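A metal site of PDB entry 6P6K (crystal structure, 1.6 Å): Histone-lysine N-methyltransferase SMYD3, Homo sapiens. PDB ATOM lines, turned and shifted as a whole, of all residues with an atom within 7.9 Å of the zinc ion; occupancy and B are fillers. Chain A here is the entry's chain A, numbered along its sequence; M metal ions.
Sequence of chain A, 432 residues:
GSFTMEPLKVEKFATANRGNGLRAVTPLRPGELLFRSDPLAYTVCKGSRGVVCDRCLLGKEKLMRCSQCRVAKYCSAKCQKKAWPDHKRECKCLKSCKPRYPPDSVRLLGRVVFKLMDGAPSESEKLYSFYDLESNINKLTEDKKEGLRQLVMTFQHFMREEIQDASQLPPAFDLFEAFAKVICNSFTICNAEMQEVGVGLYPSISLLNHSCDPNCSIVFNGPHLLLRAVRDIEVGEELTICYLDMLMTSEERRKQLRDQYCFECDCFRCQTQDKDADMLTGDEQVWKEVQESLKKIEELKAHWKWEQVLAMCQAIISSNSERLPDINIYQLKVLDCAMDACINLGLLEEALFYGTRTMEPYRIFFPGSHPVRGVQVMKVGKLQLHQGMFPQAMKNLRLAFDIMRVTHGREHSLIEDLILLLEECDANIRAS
The side-chain sulfur of Cys 56 sits close to the backbone NH of Leu 58 (3.6 Å).
The side-chain hydroxyl (OG) of Ser 76 lies within hydrogen-bond range of the backbone NH (N) of Cys 79, at 3.0 Å.
OG of Ser 76 lies close to SG of Cys 75 (3.3 Å).
The backbone NH (N) of Arg 55 sits close to the side-chain sulfur (SG) of Cys 53, 3.3 Å away.
O of Leu 58 lies within hydrogen-bond range of N of Cys 53.
The side-chain sulfur (SG) of Cys 56 binds the zinc ion, at 2.3 Å.
SG of Cys 79 binds the zinc ion (2.3 Å).
The side-chain sulfur (SG) of Cys 75 binds the zinc ion, 2.3 Å away.
The zinc ion is bound by the side-chain sulfur (SG) of Cys 53, 2.6 Å away.
The zinc ion has four donor atoms within binding distance.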
ATOM      1  N   VAL A  52      -0.193 -25.665  26.660  1.00  0.00           N
ATOM      2  CA  VAL A  52      -1.392 -25.129  26.035  1.00  0.00           C
ATOM      3  C   VAL A  52      -1.438 -23.625  26.225  1.00  0.00           C
ATOM      4  O   VAL A  52      -0.848 -23.057  27.148  1.00  0.00           O
ATOM      5  CB  VAL A  52      -2.693 -25.772  26.582  1.00  0.00           C
ATOM      6  CG1 VAL A  52      -2.739 -27.253  26.235  1.00  0.00           C
ATOM      7  CG2 VAL A  52      -2.812 -25.540  28.069  1.00  0.00           C
ATOM      8  N   CYS A  53      -2.157 -22.969  25.315  1.00  0.00           N
ATOM      9  CA  CYS A  53      -2.328 -21.522  25.375  1.00  0.00           C
ATOM     10  C   CYS A  53      -3.023 -21.124  26.671  1.00  0.00           C
ATOM     11  O   CYS A  53      -4.008 -21.750  27.093  1.00  0.00           O
ATOM     12  CB  CYS A  53      -3.128 -21.032  24.178  1.00  0.00           C
ATOM     13  SG  CYS A  53      -3.542 -19.262  24.198  1.00  0.00           S
ATOM     14  N   ASP A  54      -2.498 -20.072  27.302  1.00  0.00           N
ATOM     15  CA  ASP A  54      -3.102 -19.542  28.525  1.00  0.00           C
ATOM     16  C   ASP A  54      -4.554 -19.156  28.324  1.00  0.00           C
ATOM     17  O   ASP A  54      -5.382 -19.305  29.228  1.00  0.00           O
ATOM     18  CB  ASP A  54      -2.345 -18.306  28.992  1.00  0.00           C
ATOM     19  CG  ASP A  54      -1.358 -18.601  30.076  1.00  0.00           C
ATOM     20  OD1 ASP A  54      -0.467 -19.439  29.853  1.00  0.00           O
ATOM     21  OD2 ASP A  54      -1.479 -17.968  31.156  1.00  0.00           O
ATOM     22  N   ARG A  55      -4.871 -18.619  27.145  1.00  0.00           N
ATOM     23  CA  ARG A  55      -6.202 -18.047  26.889  1.00  0.00           C
ATOM     24  C   ARG A  55      -7.187 -19.127  26.442  1.00  0.00           C
ATOM     25  O   ARG A  55      -8.149 -19.442  27.135  1.00  0.00           O
ATOM     26  CB  ARG A  55      -6.079 -16.952  25.835  1.00  0.00           C
ATOM     27  CG  ARG A  55      -7.368 -16.200  25.547  1.00  0.00           C
ATOM     28  CD  ARG A  55      -7.753 -15.342  26.736  1.00  0.00           C
ATOM     29  NE  ARG A  55      -8.933 -14.519  26.460  1.00  0.00           N
ATOM     30  CZ  ARG A  55      -9.487 -13.713  27.349  1.00  0.00           C
ATOM     31  NH1 ARG A  55      -8.986 -13.618  28.568  1.00  0.00           N
ATOM     32  NH2 ARG A  55     -10.556 -13.001  27.018  1.00  0.00           N
ATOM     33  N   CYS A  56      -6.941 -19.700  25.256  1.00  0.00           N
ATOM     34  CA  CYS A  56      -7.880 -20.615  24.652  1.00  0.00           C
ATOM     35  C   CYS A  56      -7.719 -22.066  25.116  1.00  0.00           C
ATOM     36  O   CYS A  56      -8.594 -22.882  24.821  1.00  0.00           O
ATOM     37  CB  CYS A  56      -7.763 -20.554  23.122  1.00  0.00           C
ATOM     38  SG  CYS A  56      -6.226 -21.202  22.451  1.00  0.00           S
ATOM     39  N   LEU A  57      -6.620 -22.382  25.811  1.00  0.00           N
ATOM     40  CA  LEU A  57      -6.374 -23.702  26.392  1.00  0.00           C
ATOM     41  C   LEU A  57      -6.184 -24.778  25.317  1.00  0.00           C
ATOM     42  O   LEU A  57      -6.452 -25.958  25.565  1.00  0.00           O
ATOM     43  CB  LEU A  57      -7.475 -24.107  27.371  1.00  0.00           C
ATOM     44  CG  LEU A  57      -7.687 -23.153  28.550  1.00  0.00           C
ATOM     45  CD1 LEU A  57      -8.832 -23.638  29.457  1.00  0.00           C
ATOM     46  CD2 LEU A  57      -6.398 -23.003  29.333  1.00  0.00           C
ATOM     47  N   LEU A  58      -5.706 -24.382  24.142  1.00  0.00           N
ATOM     48  CA  LEU A  58      -5.391 -25.314  23.066  1.00  0.00           C
ATOM     49  C   LEU A  58      -3.890 -25.561  23.022  1.00  0.00           C
ATOM     50  O   LEU A  58      -3.084 -24.688  23.333  1.00  0.00           O
ATOM     51  CB  LEU A  58      -5.858 -24.774  21.716  1.00  0.00           C
ATOM     52  CG  LEU A  58      -7.358 -24.484  21.572  1.00  0.00           C
ATOM     53  CD1 LEU A  58      -7.646 -23.897  20.192  1.00  0.00           C
ATOM     54  CD2 LEU A  58      -8.174 -25.741  21.815  1.00  0.00           C
ATOM     55  N   GLY A  59      -3.522 -26.774  22.607  1.00  0.00           N
ATOM     56  CA  GLY A  59      -2.121 -27.185  22.652  1.00  0.00           C
ATOM     57  C   GLY A  59      -1.314 -26.668  21.468  1.00  0.00           C
ATOM     58  O   GLY A  59      -1.744 -26.718  20.317  1.00  0.00           O
ATOM     59  N   LEU A  63       4.564 -22.224  21.560  1.00  0.00           N
ATOM     60  CA  LEU A  63       3.853 -21.110  22.173  1.00  0.00           C
ATOM     61  C   LEU A  63       4.781 -19.907  22.348  1.00  0.00           C
ATOM     62  O   LEU A  63       5.986 -20.062  22.544  1.00  0.00           O
ATOM     63  CB  LEU A  63       3.277 -21.511  23.538  1.00  0.00           C
ATOM     64  CG  LEU A  63       2.253 -22.647  23.540  1.00  0.00           C
ATOM     65  CD1 LEU A  63       1.773 -22.895  24.955  1.00  0.00           C
ATOM     66  CD2 LEU A  63       1.092 -22.331  22.611  1.00  0.00           C
ATOM     67  N   LYS A  73       2.048 -18.192  28.342  1.00  0.00           N
ATOM     68  CA  LYS A  73       2.379 -18.544  26.973  1.00  0.00           C
ATOM     69  C   LYS A  73       1.114 -18.659  26.151  1.00  0.00           C
ATOM     70  O   LYS A  73       0.051 -19.034  26.661  1.00  0.00           O
ATOM     71  CB  LYS A  73       3.185 -19.857  26.914  1.00  0.00           C
ATOM     72  CG  LYS A  73       4.470 -19.788  27.725  1.00  0.00           C
ATOM     73  CD  LYS A  73       5.403 -20.947  27.415  1.00  0.00           C
ATOM     74  CE  LYS A  73       6.627 -20.917  28.333  1.00  0.00           C
ATOM     75  NZ  LYS A  73       7.422 -22.166  28.242  1.00  0.00           N
ATOM     76  N   TYR A  74       1.211 -18.332  24.859  1.00  0.00           N
ATOM     77  CA  TYR A  74       0.027 -18.172  24.028  1.00  0.00           C
ATOM     78  C   TYR A  74       0.206 -18.826  22.669  1.00  0.00           C
ATOM     79  O   TYR A  74       1.324 -18.931  22.149  1.00  0.00           O
ATOM     80  CB  TYR A  74      -0.305 -16.693  23.847  1.00  0.00           C
ATOM     81  CG  TYR A  74      -0.501 -15.960  25.155  1.00  0.00           C
ATOM     82  CD1 TYR A  74      -1.707 -16.019  25.831  1.00  0.00           C
ATOM     83  CD2 TYR A  74       0.533 -15.211  25.720  1.00  0.00           C
ATOM     84  CE1 TYR A  74      -1.894 -15.345  27.035  1.00  0.00           C
ATOM     85  CE2 TYR A  74       0.354 -14.536  26.912  1.00  0.00           C
ATOM     86  CZ  TYR A  74      -0.860 -14.614  27.564  1.00  0.00           C
ATOM     87  OH  TYR A  74      -1.039 -13.943  28.747  1.00  0.00           O
ATOM     88  N   CYS A  75      -0.915 -19.244  22.097  1.00  0.00           N
ATOM     89  CA  CYS A  75      -0.965 -19.889  20.798  1.00  0.00           C
ATOM     90  C   CYS A  75      -0.878 -18.894  19.647  1.00  0.00           C
ATOM     91  O   CYS A  75      -0.528 -19.287  18.521  1.00  0.00           O
ATOM     92  CB  CYS A  75      -2.262 -20.690  20.666  1.00  0.00           C
ATOM     93  SG  CYS A  75      -3.744 -19.687  20.275  1.00  0.00           S
ATOM     94  N   SER A  76      -1.204 -17.632  19.895  1.00  0.00           N
ATOM     95  CA  SER A  76      -1.332 -16.654  18.816  1.00  0.00           C
ATOM     96  C   SER A  76      -1.176 -15.266  19.389  1.00  0.00           C
ATOM     97  O   SER A  76      -1.273 -15.059  20.599  1.00  0.00           O
ATOM     98  CB  SER A  76      -2.686 -16.790  18.103  1.00  0.00           C
ATOM     99  OG  SER A  76      -3.751 -16.591  19.034  1.00  0.00           O
ATOM    100  N   ALA A  77      -0.929 -14.313  18.494  1.00  0.00           N
ATOM    101  CA  ALA A  77      -0.943 -12.910  18.901  1.00  0.00           C
ATOM    102  C   ALA A  77      -2.346 -12.497  19.344  1.00  0.00           C
ATOM    103  O   ALA A  77      -2.498 -11.698  20.276  1.00  0.00           O
ATOM    104  CB  ALA A  77      -0.436 -12.024  17.766  1.00  0.00           C
ATOM    105  N   LYS A  78      -3.376 -13.037  18.678  1.00  0.00           N
ATOM    106  CA  LYS A  78      -4.745 -12.747  19.081  1.00  0.00           C
ATOM    107  C   LYS A  78      -4.971 -13.155  20.533  1.00  0.00           C
ATOM    108  O   LYS A  78      -5.551 -12.396  21.322  1.00  0.00           O
ATOM    109  CB  LYS A  78      -5.731 -13.474  18.162  1.00  0.00           C
ATOM    110  CG  LYS A  78      -7.191 -13.228  18.485  1.00  0.00           C
ATOM    111  CD  LYS A  78      -8.113 -14.097  17.636  1.00  0.00           C
ATOM    112  N   CYS A  79      -4.486 -14.333  20.915  1.00  0.00           N
ATOM    113  CA  CYS A  79      -4.711 -14.802  22.274  1.00  0.00           C
ATOM    114  C   CYS A  79      -3.862 -14.049  23.279  1.00  0.00           C
ATOM    115  O   CYS A  79      -4.334 -13.740  24.366  1.00  0.00           O
ATOM    116  CB  CYS A  79      -4.462 -16.300  22.374  1.00  0.00           C
ATOM    117  SG  CYS A  79      -5.937 -17.248  21.921  1.00  0.00           S
ATOM    118  N   GLN A  80      -2.594 -13.743  22.939  1.00  0.00           N
ATOM    119  CA  GLN A  80      -1.783 -12.952  23.858  1.00  0.00           C
ATOM    120  C   GLN A  80      -2.394 -11.572  24.077  1.00  0.00           C
ATOM    121  O   GLN A  80      -2.480 -11.101  25.214  1.00  0.00           O
ATOM    122  CB  GLN A  80      -0.346 -12.817  23.349  1.00  0.00           C
ATOM    123  CG  GLN A  80       0.516 -11.970  24.274  1.00  0.00           C
ATOM    124  CD  GLN A  80       2.003 -12.036  23.986  1.00  0.00           C
ATOM    125  OE1 GLN A  80       2.450 -12.818  23.151  1.00  0.00           O
ATOM    126  NE2 GLN A  80       2.773 -11.214  24.689  1.00  0.00           N
HETATM  127 ZN    ZN M   1      -5.032 -19.311  22.128  1.00  0.00          ZN
